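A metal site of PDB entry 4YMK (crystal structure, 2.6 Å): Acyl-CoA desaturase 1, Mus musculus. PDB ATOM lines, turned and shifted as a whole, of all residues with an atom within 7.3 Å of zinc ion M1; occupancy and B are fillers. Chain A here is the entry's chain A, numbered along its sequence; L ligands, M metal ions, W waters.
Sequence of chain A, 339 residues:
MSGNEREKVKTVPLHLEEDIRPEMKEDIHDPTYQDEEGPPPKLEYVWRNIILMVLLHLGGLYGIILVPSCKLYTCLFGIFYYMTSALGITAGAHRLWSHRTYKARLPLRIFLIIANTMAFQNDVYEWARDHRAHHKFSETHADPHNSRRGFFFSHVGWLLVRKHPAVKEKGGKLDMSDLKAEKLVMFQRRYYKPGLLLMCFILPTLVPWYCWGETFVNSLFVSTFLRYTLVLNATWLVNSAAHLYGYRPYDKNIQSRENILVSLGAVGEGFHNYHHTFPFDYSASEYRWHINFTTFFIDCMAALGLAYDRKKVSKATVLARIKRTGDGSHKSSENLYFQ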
ATOM      1  N   HIS A 131       9.705 -20.920 -28.945  1.00  0.00           N
ATOM      2  CA  HIS A 131       9.594 -21.930 -27.904  1.00  0.00           C
ATOM      3  C   HIS A 131       8.193 -22.520 -27.811  1.00  0.00           C
ATOM      4  O   HIS A 131       8.033 -23.719 -27.618  1.00  0.00           O
ATOM      5  CB  HIS A 131      10.013 -21.366 -26.558  1.00  0.00           C
ATOM      6  CG  HIS A 131      10.174 -22.413 -25.500  1.00  0.00           C
ATOM      7  ND1 HIS A 131      11.086 -23.438 -25.604  1.00  0.00           N
ATOM      8  CD2 HIS A 131       9.508 -22.610 -24.337  1.00  0.00           C
ATOM      9  CE1 HIS A 131      10.990 -24.214 -24.542  1.00  0.00           C
ATOM     10  NE2 HIS A 131      10.044 -23.741 -23.750  1.00  0.00           N
ATOM     11  N   HIS A 134       7.917 -24.790 -30.427  1.00  0.00           N
ATOM     12  CA  HIS A 134       8.732 -25.951 -30.084  1.00  0.00           C
ATOM     13  C   HIS A 134       7.967 -26.948 -29.221  1.00  0.00           C
ATOM     14  O   HIS A 134       8.231 -28.148 -29.260  1.00  0.00           O
ATOM     15  CB  HIS A 134      10.010 -25.516 -29.365  1.00  0.00           C
ATOM     16  CG  HIS A 134      10.763 -26.636 -28.727  1.00  0.00           C
ATOM     17  ND1 HIS A 134      11.448 -27.584 -29.454  1.00  0.00           N
ATOM     18  CD2 HIS A 134      10.946 -26.958 -27.424  1.00  0.00           C
ATOM     19  CE1 HIS A 134      12.012 -28.451 -28.634  1.00  0.00           C
ATOM     20  NE2 HIS A 134      11.721 -28.099 -27.393  1.00  0.00           N
ATOM     21  N   HIS A 135       7.004 -26.443 -28.445  1.00  0.00           N
ATOM     22  CA  HIS A 135       6.209 -27.289 -27.560  1.00  0.00           C
ATOM     23  C   HIS A 135       4.954 -27.832 -28.251  1.00  0.00           C
ATOM     24  O   HIS A 135       4.642 -29.010 -28.132  1.00  0.00           O
ATOM     25  CB  HIS A 135       5.806 -26.515 -26.305  1.00  0.00           C
ATOM     26  CG  HIS A 135       6.819 -26.582 -25.200  1.00  0.00           C
ATOM     27  ND1 HIS A 135       6.749 -27.514 -24.192  1.00  0.00           N
ATOM     28  CD2 HIS A 135       7.911 -25.828 -24.958  1.00  0.00           C
ATOM     29  CE1 HIS A 135       7.769 -27.344 -23.372  1.00  0.00           C
ATOM     30  NE2 HIS A 135       8.489 -26.323 -23.811  1.00  0.00           N
ATOM     31  N   SER A 138       6.236 -30.171 -31.444  1.00  0.00           N
ATOM     32  CA  SER A 138       7.511 -30.820 -31.172  1.00  0.00           C
ATOM     33  C   SER A 138       7.793 -31.955 -32.159  1.00  0.00           C
ATOM     34  O   SER A 138       6.883 -32.662 -32.578  1.00  0.00           O
ATOM     35  CB  SER A 138       7.524 -31.345 -29.729  1.00  0.00           C
ATOM     36  OG  SER A 138       8.797 -31.841 -29.383  1.00  0.00           O
ATOM     37  N   GLU A 139       9.070 -32.112 -32.511  1.00  0.00           N
ATOM     38  CA  GLU A 139       9.531 -33.150 -33.430  1.00  0.00           C
ATOM     39  C   GLU A 139       8.874 -33.099 -34.805  1.00  0.00           C
ATOM     40  O   GLU A 139       8.714 -34.118 -35.470  1.00  0.00           O
ATOM     41  CB  GLU A 139       9.328 -34.538 -32.803  1.00  0.00           C
ATOM     42  CG  GLU A 139      10.478 -35.002 -31.928  1.00  0.00           C
ATOM     43  CD  GLU A 139      10.580 -34.233 -30.630  1.00  0.00           C
ATOM     44  OE1 GLU A 139       9.530 -33.965 -30.015  1.00  0.00           O
ATOM     45  OE2 GLU A 139      11.716 -33.902 -30.226  1.00  0.00           O
ATOM     46  N   ASP A 143       8.793 -27.264 -35.581  1.00  0.00           N
ATOM     47  CA  ASP A 143       9.673 -27.125 -34.435  1.00  0.00           C
ATOM     48  C   ASP A 143      11.024 -26.549 -34.877  1.00  0.00           C
ATOM     49  O   ASP A 143      11.751 -27.197 -35.627  1.00  0.00           O
ATOM     50  CB  ASP A 143       9.868 -28.477 -33.743  1.00  0.00           C
ATOM     51  CG  ASP A 143      10.823 -28.418 -32.562  1.00  0.00           C
ATOM     52  OD1 ASP A 143      11.031 -27.315 -32.006  1.00  0.00           O
ATOM     53  OD2 ASP A 143      11.365 -29.471 -32.182  1.00  0.00           O
ATOM     54  N   HIS A 145      13.885 -26.249 -33.600  1.00  0.00           N
ATOM     55  CA  HIS A 145      15.046 -27.113 -33.384  1.00  0.00           C
ATOM     56  C   HIS A 145      14.653 -28.579 -33.442  1.00  0.00           C
ATOM     57  O   HIS A 145      14.967 -29.349 -32.530  1.00  0.00           O
ATOM     58  CB  HIS A 145      15.719 -26.796 -32.039  1.00  0.00           C
ATOM     59  CG  HIS A 145      14.976 -25.813 -31.199  1.00  0.00           C
ATOM     60  ND1 HIS A 145      15.026 -24.452 -31.419  1.00  0.00           N
ATOM     61  CD2 HIS A 145      14.174 -25.993 -30.114  1.00  0.00           C
ATOM     62  CE1 HIS A 145      14.276 -23.841 -30.512  1.00  0.00           C
ATOM     63  NE2 HIS A 145      13.755 -24.744 -29.713  1.00  0.00           N
ATOM     64  N   VAL A 238      19.810 -28.518 -23.986  1.00  0.00           N
ATOM     65  CA  VAL A 238      18.420 -28.792 -23.658  1.00  0.00           C
ATOM     66  C   VAL A 238      17.659 -29.177 -24.921  1.00  0.00           C
ATOM     67  O   VAL A 238      16.670 -29.914 -24.866  1.00  0.00           O
ATOM     68  CB  VAL A 238      17.768 -27.591 -22.943  1.00  0.00           C
ATOM     69  CG1 VAL A 238      16.364 -27.937 -22.466  1.00  0.00           C
ATOM     70  CG2 VAL A 238      18.619 -27.141 -21.769  1.00  0.00           C
ATOM     71  N   ASN A 239      18.117 -28.677 -26.064  1.00  0.00           N
ATOM     72  CA  ASN A 239      17.470 -28.975 -27.341  1.00  0.00           C
ATOM     73  C   ASN A 239      18.016 -30.248 -27.991  1.00  0.00           C
ATOM     74  O   ASN A 239      17.284 -30.962 -28.680  1.00  0.00           O
ATOM     75  CB  ASN A 239      17.645 -27.805 -28.313  1.00  0.00           C
ATOM     76  CG  ASN A 239      16.868 -26.582 -27.892  1.00  0.00           C
ATOM     77  OD1 ASN A 239      17.368 -25.460 -27.970  1.00  0.00           O
ATOM     78  ND2 ASN A 239      15.635 -26.789 -27.461  1.00  0.00           N
ATOM     79  N   SER A 240      19.300 -30.529 -27.771  1.00  0.00           N
ATOM     80  CA  SER A 240      19.938 -31.684 -28.396  1.00  0.00           C
ATOM     81  C   SER A 240      19.976 -32.895 -27.456  1.00  0.00           C
ATOM     82  O   SER A 240      19.253 -33.865 -27.653  1.00  0.00           O
ATOM     83  CB  SER A 240      21.353 -31.323 -28.851  1.00  0.00           C
ATOM     84  OG  SER A 240      22.145 -30.847 -27.769  1.00  0.00           O
ATOM     85  N   ALA A 242      18.965 -33.359 -24.361  1.00  0.00           N
ATOM     86  CA  ALA A 242      17.739 -33.613 -23.610  1.00  0.00           C
ATOM     87  C   ALA A 242      16.602 -34.110 -24.518  1.00  0.00           C
ATOM     88  O   ALA A 242      15.486 -34.306 -24.055  1.00  0.00           O
ATOM     89  CB  ALA A 242      17.308 -32.360 -22.866  1.00  0.00           C
ATOM     90  N   HIS A 243      16.909 -34.295 -25.804  1.00  0.00           N
ATOM     91  CA  HIS A 243      15.945 -34.866 -26.747  1.00  0.00           C
ATOM     92  C   HIS A 243      16.478 -36.174 -27.325  1.00  0.00           C
ATOM     93  O   HIS A 243      15.925 -36.687 -28.303  1.00  0.00           O
ATOM     94  CB  HIS A 243      15.644 -33.883 -27.871  1.00  0.00           C
ATOM     95  CG  HIS A 243      14.564 -32.897 -27.556  1.00  0.00           C
ATOM     96  ND1 HIS A 243      13.275 -33.041 -28.019  1.00  0.00           N
ATOM     97  CD2 HIS A 243      14.579 -31.760 -26.818  1.00  0.00           C
ATOM     98  CE1 HIS A 243      12.534 -32.032 -27.577  1.00  0.00           C
ATOM     99  NE2 HIS A 243      13.301 -31.244 -26.845  1.00  0.00           N
ATOM    100  N   SER A 256      11.443 -36.139 -25.433  1.00  0.00           N
ATOM    101  CA  SER A 256      12.005 -35.361 -24.335  1.00  0.00           C
ATOM    102  C   SER A 256      12.550 -36.293 -23.263  1.00  0.00           C
ATOM    103  O   SER A 256      11.901 -37.277 -22.901  1.00  0.00           O
ATOM    104  CB  SER A 256      10.963 -34.424 -23.745  1.00  0.00           C
ATOM    105  OG  SER A 256      10.238 -33.774 -24.787  1.00  0.00           O
ATOM    106  N   HIS A 272      13.648 -32.606 -18.902  1.00  0.00           N
ATOM    107  CA  HIS A 272      12.921 -32.188 -20.082  1.00  0.00           C
ATOM    108  C   HIS A 272      11.718 -33.077 -20.393  1.00  0.00           C
ATOM    109  O   HIS A 272      10.752 -32.628 -21.023  1.00  0.00           O
ATOM    110  CB  HIS A 272      13.861 -32.162 -21.286  1.00  0.00           C
ATOM    111  CG  HIS A 272      13.520 -31.113 -22.300  1.00  0.00           C
ATOM    112  ND1 HIS A 272      13.125 -29.836 -21.943  1.00  0.00           N
ATOM    113  CD2 HIS A 272      13.509 -31.148 -23.650  1.00  0.00           C
ATOM    114  CE1 HIS A 272      12.887 -29.134 -23.040  1.00  0.00           C
ATOM    115  NE2 HIS A 272      13.111 -29.905 -24.089  1.00  0.00           N
ATOM    116  N   HIS A 275       9.044 -31.636 -18.227  1.00  0.00           N
ATOM    117  CA  HIS A 275       8.680 -30.303 -18.692  1.00  0.00           C
ATOM    118  C   HIS A 275       7.786 -30.317 -19.922  1.00  0.00           C
ATOM    119  O   HIS A 275       6.814 -29.575 -20.002  1.00  0.00           O
ATOM    120  CB  HIS A 275       9.939 -29.477 -18.987  1.00  0.00           C
ATOM    121  CG  HIS A 275       9.652 -28.145 -19.592  1.00  0.00           C
ATOM    122  ND1 HIS A 275       8.903 -27.190 -18.941  1.00  0.00           N
ATOM    123  CD2 HIS A 275       9.984 -27.614 -20.792  1.00  0.00           C
ATOM    124  CE1 HIS A 275       8.803 -26.114 -19.706  1.00  0.00           C
ATOM    125  NE2 HIS A 275       9.444 -26.352 -20.844  1.00  0.00           N
ATOM    126  N   HIS A 276       8.106 -31.174 -20.895  1.00  0.00           N
ATOM    127  CA  HIS A 276       7.282 -31.274 -22.100  1.00  0.00           C
ATOM    128  C   HIS A 276       5.928 -31.898 -21.786  1.00  0.00           C
ATOM    129  O   HIS A 276       4.940 -31.642 -22.474  1.00  0.00           O
ATOM    130  CB  HIS A 276       7.998 -32.069 -23.189  1.00  0.00           C
ATOM    131  CG  HIS A 276       8.780 -31.225 -24.142  1.00  0.00           C
ATOM    132  ND1 HIS A 276       8.210 -30.650 -25.257  1.00  0.00           N
ATOM    133  CD2 HIS A 276      10.073 -30.836 -24.133  1.00  0.00           C
ATOM    134  CE1 HIS A 276       9.132 -29.960 -25.905  1.00  0.00           C
ATOM    135  NE2 HIS A 276      10.268 -30.060 -25.252  1.00  0.00           N
HETATM  136  C1  LIG L   1      19.884 -18.648 -29.500  1.00  0.00           C
HETATM  137  C2  LIG L   1      18.602 -18.997 -28.791  1.00  0.00           C
HETATM  138  O1  LIG L   1      20.842 -19.381 -29.438  1.00  0.00           O
HETATM  139  C3  LIG L   1      18.294 -20.488 -28.946  1.00  0.00           C
HETATM  140  C4  LIG L   1      18.317 -21.177 -27.581  1.00  0.00           C
HETATM  141  C5  LIG L   1      16.908 -21.210 -26.994  1.00  0.00           C
HETATM  142  C6  LIG L   1      16.334 -22.621 -27.047  1.00  0.00           C
HETATM  143  C7  LIG L   1      16.168 -23.189 -25.633  1.00  0.00           C
HETATM  144  C8  LIG L   1      14.818 -23.915 -25.526  1.00  0.00           C
HETATM  145  C9  LIG L   1      14.971 -25.154 -24.642  1.00  0.00           C
HETATM  146  C10 LIG L   1      14.100 -25.026 -23.388  1.00  0.00           C
HETATM  147  C11 LIG L   1      14.640 -23.941 -22.466  1.00  0.00           C
HETATM  148  C12 LIG L   1      16.015 -24.340 -21.912  1.00  0.00           C
HETATM  149  C13 LIG L   1      16.662 -23.125 -21.225  1.00  0.00           C
HETATM  150  C14 LIG L   1      18.075 -23.491 -20.746  1.00  0.00           C
HETATM  151  C15 LIG L   1      18.821 -22.221 -20.339  1.00  0.00           C
HETATM  152  C16 LIG L   1      20.210 -22.578 -19.816  1.00  0.00           C
HETATM  153  C17 LIG L   1      20.979 -21.295 -19.460  1.00  0.00           C
HETATM  154  C18 LIG L   1      22.377 -21.660 -18.964  1.00  0.00           C
HETATM  155  N1  LIG L   1       6.671 -18.226 -35.301  1.00  0.00           N
HETATM  156  O2  LIG L   1      14.134 -15.612 -38.010  1.00  0.00           O
HETATM  157  P1  LIG L   1      13.681 -15.248 -39.373  1.00  0.00           P
HETATM  158  C19 LIG L   1       8.524 -15.343 -39.162  1.00  0.00           C
HETATM  159  S1  LIG L   1      19.974 -17.182 -30.391  1.00  0.00           S
HETATM  160  C20 LIG L   1       6.022 -17.432 -36.135  1.00  0.00           C
HETATM  161  O3  LIG L   1      14.576 -14.051 -39.964  1.00  0.00           O
HETATM  162  P2  LIG L   1      14.919 -17.026 -41.380  1.00  0.00           P
HETATM  163  C21 LIG L   1       8.230 -13.923 -38.601  1.00  0.00           C
HETATM  164  O4  LIG L   1       7.231 -13.278 -39.377  1.00  0.00           O
HETATM  165  C22 LIG L   1      21.742 -16.839 -30.290  1.00  0.00           C
HETATM  166  N2  LIG L   1       6.631 -16.755 -37.079  1.00  0.00           N
HETATM  167  O5  LIG L   1      13.802 -16.535 -40.330  1.00  0.00           O
HETATM  168  C23 LIG L   1       9.599 -13.216 -38.773  1.00  0.00           C
HETATM  169  O6  LIG L   1       9.431 -11.803 -38.878  1.00  0.00           O
HETATM  170  P3  LIG L   1       9.844 -10.777 -37.704  1.00  0.00           P
HETATM  171  C24 LIG L   1      21.999 -15.423 -30.833  1.00  0.00           C
HETATM  172  C25 LIG L   1       7.948 -16.846 -37.222  1.00  0.00           C
HETATM  173  O7  LIG L   1      15.102 -15.914 -42.517  1.00  0.00           O
HETATM  174  C26 LIG L   1      10.079 -13.825 -40.097  1.00  0.00           C
HETATM  175  O8  LIG L   1       9.636 -15.197 -40.079  1.00  0.00           O
HETATM  176  N3  LIG L   1      21.018 -15.136 -31.887  1.00  0.00           N
HETATM  177  C27 LIG L   1       8.686 -17.664 -36.354  1.00  0.00           C
HETATM  178  O9  LIG L   1      14.502 -18.323 -41.974  1.00  0.00           O
HETATM  179  C28 LIG L   1      11.601 -13.783 -40.175  1.00  0.00           C
HETATM  180  O10 LIG L   1      12.138 -14.793 -39.321  1.00  0.00           O
HETATM  181  C29 LIG L   1      21.288 -15.503 -33.162  1.00  0.00           C
HETATM  182  O11 LIG L   1      22.327 -16.057 -33.434  1.00  0.00           O
HETATM  183  C30 LIG L   1       7.986 -18.377 -35.361  1.00  0.00           C
HETATM  184  N4  LIG L   1       8.645 -19.201 -34.471  1.00  0.00           N
HETATM  185  O12 LIG L   1      16.312 -17.224 -40.588  1.00  0.00           O
HETATM  186  C31 LIG L   1      20.283 -15.225 -34.263  1.00  0.00           C
HETATM  187  N5  LIG L   1       9.992 -17.560 -36.722  1.00  0.00           N
HETATM  188  O13 LIG L   1       9.789 -11.526 -36.279  1.00  0.00           O
HETATM  189  C32 LIG L   1      20.502 -16.263 -35.364  1.00  0.00           C
HETATM  190  C33 LIG L   1      10.084 -16.749 -37.730  1.00  0.00           C
HETATM  191  O14 LIG L   1      11.343 -10.262 -37.964  1.00  0.00           O
HETATM  192  N6  LIG L   1      19.226 -16.637 -36.003  1.00  0.00           N
HETATM  193  N7  LIG L   1       8.856 -16.269 -38.079  1.00  0.00           N
HETATM  194  O15 LIG L   1       8.912  -9.631 -37.708  1.00  0.00           O
HETATM  195  C34 LIG L   1      18.933 -16.157 -37.234  1.00  0.00           C
HETATM  196  O16 LIG L   1      19.723 -15.423 -37.772  1.00  0.00           O
HETATM  197  C35 LIG L   1      17.638 -16.527 -37.924  1.00  0.00           C
HETATM  198  O17 LIG L   1      16.603 -16.701 -36.943  1.00  0.00           O
HETATM  199  C36 LIG L   1      17.771 -17.802 -38.761  1.00  0.00           C
HETATM  200  C37 LIG L   1      16.433 -18.074 -39.450  1.00  0.00           C
HETATM  201  C38 LIG L   1      18.132 -18.998 -37.881  1.00  0.00           C
HETATM  202  C39 LIG L   1      18.836 -17.618 -39.833  1.00  0.00           C
HETATM  203 ZN    ZN M   1      12.373 -29.511 -25.872  1.00  0.00          ZN
HETATM  204 ZN    ZN M   2       9.537 -25.024 -22.311  1.00  0.00          ZN
HETATM  205  O   HOH W   1      14.225 -28.310 -25.862  1.00  0.00           O
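The side-chain carboxylate of Asp 143 is in hydrogen-bond range of a ring nitrogen (ND1) of His 134.
ND1 of His 243 is in hydrogen-bond range of OE2 of Glu 139 (2.8 Å).
A ring nitrogen (NE2) of His 272 binds zinc ion M1, 2.0 Å away.
Zinc ion M1 is bound by NE2 of His 134 (2.2 Å).
Zinc ion M1 is bound by NE2 of His 243.
Water W1 binds zinc ion M1 (2.2 Å).
Zinc ion M1 is bound by NE2 of His 276, 2.3 Å away.
Water W1 bridges ND2 of Asn 239 (2.6 Å) and O of Val 238 (3.1 Å).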
